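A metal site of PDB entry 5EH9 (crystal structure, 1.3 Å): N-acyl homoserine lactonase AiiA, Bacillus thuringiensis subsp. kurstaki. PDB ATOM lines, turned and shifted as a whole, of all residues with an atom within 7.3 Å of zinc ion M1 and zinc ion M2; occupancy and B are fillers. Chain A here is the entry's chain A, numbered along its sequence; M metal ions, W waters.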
ATOM      1  N   LEU A  19     -23.088 -18.206 -19.420  1.00  0.00           N
ATOM      2  CA  LEU A  19     -22.282 -19.364 -19.756  1.00  0.00           C
ATOM      3  C   LEU A  19     -22.031 -20.166 -18.481  1.00  0.00           C
ATOM      4  O   LEU A  19     -21.965 -19.627 -17.396  1.00  0.00           O
ATOM      5  CB  LEU A  19     -20.943 -18.896 -20.316  1.00  0.00           C
ATOM      6  CG  LEU A  19     -20.794 -18.203 -21.655  1.00  0.00           C
ATOM      7  CD1 LEU A  19     -19.270 -18.095 -21.967  1.00  0.00           C
ATOM      8  CD2 LEU A  19     -21.550 -18.844 -22.828  1.00  0.00           C
ATOM      9  N   PRO A  37     -20.697 -10.190 -19.213  1.00  0.00           N
ATOM     10  CA  PRO A  37     -20.904  -9.038 -20.060  1.00  0.00           C
ATOM     11  C   PRO A  37     -20.633  -9.344 -21.527  1.00  0.00           C
ATOM     12  O   PRO A  37     -19.680 -10.117 -21.820  1.00  0.00           O
ATOM     13  CB  PRO A  37     -19.948  -8.034 -19.552  1.00  0.00           C
ATOM     14  CG  PRO A  37     -18.803  -8.843 -18.994  1.00  0.00           C
ATOM     15  CD  PRO A  37     -19.470 -10.063 -18.395  1.00  0.00           C
ATOM     16  N   VAL A  38     -21.381  -8.760 -22.445  1.00  0.00           N
ATOM     17  CA  VAL A  38     -21.074  -8.693 -23.840  1.00  0.00           C
ATOM     18  C   VAL A  38     -20.752  -7.245 -24.128  1.00  0.00           C
ATOM     19  O   VAL A  38     -21.475  -6.330 -23.734  1.00  0.00           O
ATOM     20  CB  VAL A  38     -22.248  -9.223 -24.697  1.00  0.00           C
ATOM     21  CG1 VAL A  38     -21.975  -8.980 -26.175  1.00  0.00           C
ATOM     22  CG2 VAL A  38     -22.490 -10.696 -24.426  1.00  0.00           C
ATOM     23  N   TRP A  39     -19.634  -7.049 -24.834  1.00  0.00           N
ATOM     24  CA  TRP A  39     -19.144  -5.697 -25.127  1.00  0.00           C
ATOM     25  C   TRP A  39     -19.020  -5.390 -26.591  1.00  0.00           C
ATOM     26  O   TRP A  39     -18.713  -6.243 -27.384  1.00  0.00           O
ATOM     27  CB  TRP A  39     -17.667  -5.567 -24.608  1.00  0.00           C
ATOM     28  CG  TRP A  39     -17.479  -5.743 -23.144  1.00  0.00           C
ATOM     29  CD1 TRP A  39     -16.862  -6.823 -22.521  1.00  0.00           C
ATOM     30  CD2 TRP A  39     -17.761  -4.796 -22.123  1.00  0.00           C
ATOM     31  NE1 TRP A  39     -16.812  -6.608 -21.167  1.00  0.00           N
ATOM     32  CE2 TRP A  39     -17.323  -5.354 -20.903  1.00  0.00           C
ATOM     33  CE3 TRP A  39     -18.284  -3.511 -22.099  1.00  0.00           C
ATOM     34  CZ2 TRP A  39     -17.406  -4.663 -19.729  1.00  0.00           C
ATOM     35  CZ3 TRP A  39     -18.398  -2.830 -20.907  1.00  0.00           C
ATOM     36  CH2 TRP A  39     -17.988  -3.405 -19.748  1.00  0.00           C
ATOM     37  N   ASP A  53     -16.737  -4.955 -32.770  1.00  0.00           N
ATOM     38  CA  ASP A  53     -17.768  -5.959 -32.517  1.00  0.00           C
ATOM     39  C   ASP A  53     -19.177  -5.336 -32.493  1.00  0.00           C
ATOM     40  O   ASP A  53     -19.373  -4.138 -32.416  1.00  0.00           O
ATOM     41  CB  ASP A  53     -17.437  -6.747 -31.251  1.00  0.00           C
ATOM     42  CG  ASP A  53     -16.228  -7.708 -31.520  1.00  0.00           C
ATOM     43  OD1 ASP A  53     -15.875  -7.917 -32.677  1.00  0.00           O
ATOM     44  OD2 ASP A  53     -15.672  -8.189 -30.482  1.00  0.00           O
ATOM     45  N   SER A 106     -13.525  -8.894 -33.894  1.00  0.00           N
ATOM     46  CA  SER A 106     -12.494  -9.627 -33.161  1.00  0.00           C
ATOM     47  C   SER A 106     -12.541 -11.086 -33.621  1.00  0.00           C
ATOM     48  O   SER A 106     -11.500 -11.754 -33.790  1.00  0.00           O
ATOM     49  CB  SER A 106     -12.730  -9.518 -31.679  1.00  0.00           C
ATOM     50  OG  SER A 106     -13.957 -10.115 -31.283  1.00  0.00           O
ATOM     51  N   HIS A 107     -13.769 -11.617 -33.754  1.00  0.00           N
ATOM     52  CA  HIS A 107     -14.003 -12.934 -34.230  1.00  0.00           C
ATOM     53  C   HIS A 107     -15.536 -13.022 -34.548  1.00  0.00           C
ATOM     54  O   HIS A 107     -16.212 -12.037 -34.334  1.00  0.00           O
ATOM     55  CB  HIS A 107     -13.558 -14.021 -33.254  1.00  0.00           C
ATOM     56  CG  HIS A 107     -14.153 -14.019 -31.900  1.00  0.00           C
ATOM     57  ND1 HIS A 107     -14.206 -12.932 -31.067  1.00  0.00           N
ATOM     58  CD2 HIS A 107     -14.660 -15.067 -31.160  1.00  0.00           C
ATOM     59  CE1 HIS A 107     -14.663 -13.295 -29.885  1.00  0.00           C
ATOM     60  NE2 HIS A 107     -14.970 -14.592 -29.928  1.00  0.00           N
ATOM     61  N   LEU A 108     -15.944 -14.146 -35.073  1.00  0.00           N
ATOM     62  CA  LEU A 108     -17.311 -14.280 -35.574  1.00  0.00           C
ATOM     63  C   LEU A 108     -18.218 -15.113 -34.722  1.00  0.00           C
ATOM     64  O   LEU A 108     -19.304 -15.528 -35.172  1.00  0.00           O
ATOM     65  CB  LEU A 108     -17.322 -14.708 -37.061  1.00  0.00           C
ATOM     66  CG  LEU A 108     -16.608 -13.756 -38.070  1.00  0.00           C
ATOM     67  CD1 LEU A 108     -16.548 -14.411 -39.425  1.00  0.00           C
ATOM     68  CD2 LEU A 108     -17.258 -12.357 -38.064  1.00  0.00           C
ATOM     69  N   HIS A 109     -17.883 -15.322 -33.474  1.00  0.00           N
ATOM     70  CA  HIS A 109     -18.828 -15.842 -32.485  1.00  0.00           C
ATOM     71  C   HIS A 109     -20.041 -14.971 -32.421  1.00  0.00           C
ATOM     72  O   HIS A 109     -20.019 -13.780 -32.624  1.00  0.00           O
ATOM     73  CB  HIS A 109     -18.185 -16.012 -31.125  1.00  0.00           C
ATOM     74  CG  HIS A 109     -17.211 -17.165 -31.086  1.00  0.00           C
ATOM     75  ND1 HIS A 109     -16.361 -17.381 -29.994  1.00  0.00           N
ATOM     76  CD2 HIS A 109     -16.965 -18.162 -31.952  1.00  0.00           C
ATOM     77  CE1 HIS A 109     -15.636 -18.469 -30.232  1.00  0.00           C
ATOM     78  NE2 HIS A 109     -15.948 -18.930 -31.412  1.00  0.00           N
ATOM     79  N   PHE A 110     -21.159 -15.578 -32.016  1.00  0.00           N
ATOM     80  CA  PHE A 110     -22.484 -14.897 -32.042  1.00  0.00           C
ATOM     81  C   PHE A 110     -22.564 -13.673 -31.207  1.00  0.00           C
ATOM     82  O   PHE A 110     -23.376 -12.764 -31.488  1.00  0.00           O
ATOM     83  CB  PHE A 110     -23.625 -15.874 -31.774  1.00  0.00           C
ATOM     84  CG  PHE A 110     -23.955 -15.985 -30.338  1.00  0.00           C
ATOM     85  CD1 PHE A 110     -23.107 -16.604 -29.431  1.00  0.00           C
ATOM     86  CD2 PHE A 110     -25.057 -15.394 -29.876  1.00  0.00           C
ATOM     87  CE1 PHE A 110     -23.401 -16.606 -28.081  1.00  0.00           C
ATOM     88  CE2 PHE A 110     -25.434 -15.516 -28.531  1.00  0.00           C
ATOM     89  CZ  PHE A 110     -24.565 -16.064 -27.623  1.00  0.00           C
ATOM     90  N   ASP A 111     -21.770 -13.654 -30.093  1.00  0.00           N
ATOM     91  CA  ASP A 111     -21.723 -12.525 -29.227  1.00  0.00           C
ATOM     92  C   ASP A 111     -20.814 -11.377 -29.616  1.00  0.00           C
ATOM     93  O   ASP A 111     -20.764 -10.369 -28.946  1.00  0.00           O
ATOM     94  CB  ASP A 111     -21.440 -12.969 -27.760  1.00  0.00           C
ATOM     95  CG  ASP A 111     -20.091 -13.724 -27.610  1.00  0.00           C
ATOM     96  OD1 ASP A 111     -19.883 -14.646 -28.455  1.00  0.00           O
ATOM     97  OD2 ASP A 111     -19.334 -13.415 -26.659  1.00  0.00           O
ATOM     98  N   HIS A 112     -20.219 -11.528 -30.797  1.00  0.00           N
ATOM     99  CA  HIS A 112     -19.338 -10.542 -31.354  1.00  0.00           C
ATOM    100  C   HIS A 112     -19.653 -10.089 -32.756  1.00  0.00           C
ATOM    101  O   HIS A 112     -19.266  -8.971 -33.133  1.00  0.00           O
ATOM    102  CB  HIS A 112     -17.869 -11.105 -31.357  1.00  0.00           C
ATOM    103  CG  HIS A 112     -17.400 -11.401 -29.999  1.00  0.00           C
ATOM    104  ND1 HIS A 112     -16.644 -10.524 -29.263  1.00  0.00           N
ATOM    105  CD2 HIS A 112     -17.629 -12.455 -29.215  1.00  0.00           C
ATOM    106  CE1 HIS A 112     -16.484 -11.004 -28.052  1.00  0.00           C
ATOM    107  NE2 HIS A 112     -17.042 -12.212 -28.016  1.00  0.00           N
ATOM    108  N   GLU A 130     -10.528 -16.652 -39.574  1.00  0.00           N
ATOM    109  CA  GLU A 130     -11.820 -16.602 -38.905  1.00  0.00           C
ATOM    110  C   GLU A 130     -12.961 -16.731 -39.901  1.00  0.00           C
ATOM    111  O   GLU A 130     -13.934 -17.477 -39.727  1.00  0.00           O
ATOM    112  CB  GLU A 130     -11.967 -15.302 -38.122  1.00  0.00           C
ATOM    113  CG  GLU A 130     -13.206 -15.292 -37.244  1.00  0.00           C
ATOM    114  CD  GLU A 130     -13.226 -16.239 -36.057  1.00  0.00           C
ATOM    115  OE1 GLU A 130     -12.127 -16.775 -35.723  1.00  0.00           O
ATOM    116  OE2 GLU A 130     -14.290 -16.455 -35.482  1.00  0.00           O
ATOM    117  N   HIS A 172      -8.782 -19.118 -29.103  1.00  0.00           N
ATOM    118  CA  HIS A 172     -10.177 -19.128 -28.673  1.00  0.00           C
ATOM    119  C   HIS A 172     -11.116 -19.416 -29.836  1.00  0.00           C
ATOM    120  O   HIS A 172     -12.127 -20.144 -29.710  1.00  0.00           O
ATOM    121  CB  HIS A 172     -10.519 -17.783 -28.033  1.00  0.00           C
ATOM    122  CG  HIS A 172     -12.024 -17.615 -27.811  1.00  0.00           C
ATOM    123  ND1 HIS A 172     -12.770 -18.253 -26.823  1.00  0.00           N
ATOM    124  CD2 HIS A 172     -12.906 -16.840 -28.474  1.00  0.00           C
ATOM    125  CE1 HIS A 172     -14.060 -17.898 -26.917  1.00  0.00           C
ATOM    126  NE2 HIS A 172     -14.150 -17.013 -27.883  1.00  0.00           N
ATOM    127  N   SER A 173     -10.805 -18.836 -31.011  1.00  0.00           N
ATOM    128  CA  SER A 173     -11.390 -19.127 -32.298  1.00  0.00           C
ATOM    129  C   SER A 173     -10.267 -19.185 -33.327  1.00  0.00           C
ATOM    130  O   SER A 173      -9.155 -18.670 -33.029  1.00  0.00           O
ATOM    131  CB  SER A 173     -12.477 -18.126 -32.658  1.00  0.00           C
ATOM    132  OG  SER A 173     -11.917 -16.857 -33.015  1.00  0.00           O
ATOM    133  N   HIS A 176      -9.156 -15.458 -34.195  1.00  0.00           N
ATOM    134  CA  HIS A 176      -9.365 -14.436 -33.236  1.00  0.00           C
ATOM    135  C   HIS A 176      -8.299 -13.325 -33.259  1.00  0.00           C
ATOM    136  O   HIS A 176      -7.079 -13.648 -33.441  1.00  0.00           O
ATOM    137  CB  HIS A 176      -9.385 -15.037 -31.789  1.00  0.00           C
ATOM    138  CG  HIS A 176      -9.729 -14.083 -30.726  1.00  0.00           C
ATOM    139  ND1 HIS A 176      -8.809 -13.247 -30.129  1.00  0.00           N
ATOM    140  CD2 HIS A 176     -10.929 -13.713 -30.188  1.00  0.00           C
ATOM    141  CE1 HIS A 176      -9.417 -12.397 -29.327  1.00  0.00           C
ATOM    142  NE2 HIS A 176     -10.724 -12.671 -29.333  1.00  0.00           N
ATOM    143  N   ILE A 193      -9.966  -9.000 -25.852  1.00  0.00           N
ATOM    144  CA  ILE A 193     -11.177  -9.640 -26.286  1.00  0.00           C
ATOM    145  C   ILE A 193     -11.086 -11.041 -25.743  1.00  0.00           C
ATOM    146  O   ILE A 193     -10.768 -11.203 -24.552  1.00  0.00           O
ATOM    147  CB  ILE A 193     -11.456  -9.507 -27.783  1.00  0.00           C
ATOM    148  CG1 ILE A 193     -11.097  -8.157 -28.355  1.00  0.00           C
ATOM    149  CG2 ILE A 193     -12.954  -9.792 -28.051  1.00  0.00           C
ATOM    150  CD1 ILE A 193     -11.877  -6.954 -27.880  1.00  0.00           C
ATOM    151  N   ASP A 194     -11.433 -12.053 -26.525  1.00  0.00           N
ATOM    152  CA  ASP A 194     -11.570 -13.405 -25.996  1.00  0.00           C
ATOM    153  C   ASP A 194     -10.304 -14.224 -26.070  1.00  0.00           C
ATOM    154  O   ASP A 194     -10.308 -15.468 -25.890  1.00  0.00           O
ATOM    155  CB  ASP A 194     -12.756 -14.124 -26.617  1.00  0.00           C
ATOM    156  CG  ASP A 194     -14.158 -13.560 -26.215  1.00  0.00           C
ATOM    157  OD1 ASP A 194     -14.150 -12.536 -25.471  1.00  0.00           O
ATOM    158  OD2 ASP A 194     -15.165 -14.182 -26.753  1.00  0.00           O
ATOM    159  N   TYR A 197     -10.845 -14.599 -21.400  1.00  0.00           N
ATOM    160  CA  TYR A 197     -12.125 -14.155 -20.829  1.00  0.00           C
ATOM    161  C   TYR A 197     -11.937 -13.331 -19.585  1.00  0.00           C
ATOM    162  O   TYR A 197     -12.561 -12.281 -19.378  1.00  0.00           O
ATOM    163  CB  TYR A 197     -13.073 -15.324 -20.475  1.00  0.00           C
ATOM    164  CG  TYR A 197     -13.723 -16.057 -21.597  1.00  0.00           C
ATOM    165  CD1 TYR A 197     -13.722 -15.668 -22.913  1.00  0.00           C
ATOM    166  CD2 TYR A 197     -14.397 -17.152 -21.313  1.00  0.00           C
ATOM    167  CE1 TYR A 197     -14.466 -16.347 -23.855  1.00  0.00           C
ATOM    168  CE2 TYR A 197     -15.092 -17.860 -22.259  1.00  0.00           C
ATOM    169  CZ  TYR A 197     -15.242 -17.437 -23.516  1.00  0.00           C
ATOM    170  OH  TYR A 197     -16.009 -18.129 -24.389  1.00  0.00           O
ATOM    171  N   ALA A 209     -12.816 -21.608 -22.466  1.00  0.00           N
ATOM    172  CA  ALA A 209     -13.419 -22.137 -23.677  1.00  0.00           C
ATOM    173  C   ALA A 209     -12.717 -21.646 -24.904  1.00  0.00           C
ATOM    174  O   ALA A 209     -12.427 -20.441 -25.016  1.00  0.00           O
ATOM    175  CB  ALA A 209     -14.847 -21.692 -23.774  1.00  0.00           C
ATOM    176  N   GLY A 237     -12.091 -10.114 -21.893  1.00  0.00           N
ATOM    177  CA  GLY A 237     -13.268 -10.186 -22.699  1.00  0.00           C
ATOM    178  C   GLY A 237     -14.576 -10.379 -21.999  1.00  0.00           C
ATOM    179  O   GLY A 237     -15.630  -9.893 -22.493  1.00  0.00           O
ATOM    180  N   HIS A 238     -14.607 -11.225 -21.002  1.00  0.00           N
ATOM    181  CA  HIS A 238     -15.897 -11.568 -20.344  1.00  0.00           C
ATOM    182  C   HIS A 238     -15.640 -11.834 -18.866  1.00  0.00           C
ATOM    183  O   HIS A 238     -15.732 -12.954 -18.348  1.00  0.00           O
ATOM    184  CB  HIS A 238     -16.464 -12.867 -20.995  1.00  0.00           C
ATOM    185  CG  HIS A 238     -16.926 -12.754 -22.410  1.00  0.00           C
ATOM    186  ND1 HIS A 238     -18.037 -12.023 -22.830  1.00  0.00           N
ATOM    187  CD2 HIS A 238     -16.516 -13.441 -23.484  1.00  0.00           C
ATOM    188  CE1 HIS A 238     -18.220 -12.207 -24.110  1.00  0.00           C
ATOM    189  NE2 HIS A 238     -17.284 -13.055 -24.533  1.00  0.00           N
HETATM  190 ZN    ZN M   1     -15.756 -15.942 -28.530  1.00  0.00          ZN
HETATM  191 ZN    ZN M   2     -17.102 -13.641 -26.526  1.00  0.00          ZN
HETATM  192  O   HOH W   1     -17.323 -15.441 -27.411  1.00  0.00           O
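Within 4 Å of zinc ion M1: His 107, His 109, His 112, His 172 and Asp 194.
The nearest printed residue that does not touch zinc ion M1 is Asp 111 (4.3 Å).
The side-chain hydroxyl (OG) of Ser 106 lies within hydrogen-bond range of a ring nitrogen (ND1) of His 107 (2.8 Å).
A ring nitrogen (ND1) of His 112 is in hydrogen-bond range of the side-chain hydroxyl (OG) of Ser 106, 3.4 Å away.
NE2 of His 176 is in hydrogen-bond range of N of Asp 194 (3.0 Å).
N of His 238 sits at hydrogen-bond distance from O of Tyr 197 (2.8 Å).
ND1 of His 238 lies within hydrogen-bond range of O of Pro 37, at 2.7 Å.
A ring nitrogen (ND1) of His 112 sits at hydrogen-bond distance from the side-chain carboxylate of Asp 53 (2.8 Å).
ND1 of His 172 sits at hydrogen-bond distance from O of Ala 209 (2.9 Å).
Water W1 is bound to zinc ion M1, at 2.0 Å.
NE2 of His 172 is bound to zinc ion M1 (2.0 Å).
NE2 of His 107 binds zinc ion M1 (2.1 Å).
ND1 of His 109 binds zinc ion M1.
OD2 of Asp 194 binds zinc ion M1.
Water W1 is bound to zinc ion M2.
The side-chain carboxylate (OD2) of Asp 194 binds zinc ion M2, 2.0 Å away.
NE2 of His 112 binds zinc ion M2 (2.1 Å).
NE2 of His 238 is bound to zinc ion M2, at 2.1 Å.
The side-chain carboxylate (OD2) of Asp 111 is bound to zinc ion M2 (2.2 Å).
Zinc ion M2 has five donor atoms within binding distance.
Of the 22 residues printed, 4 come within 4 Å of zinc ion M2.
The nearest printed residue that does not touch zinc ion M2 is His 107 (4.1 Å).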
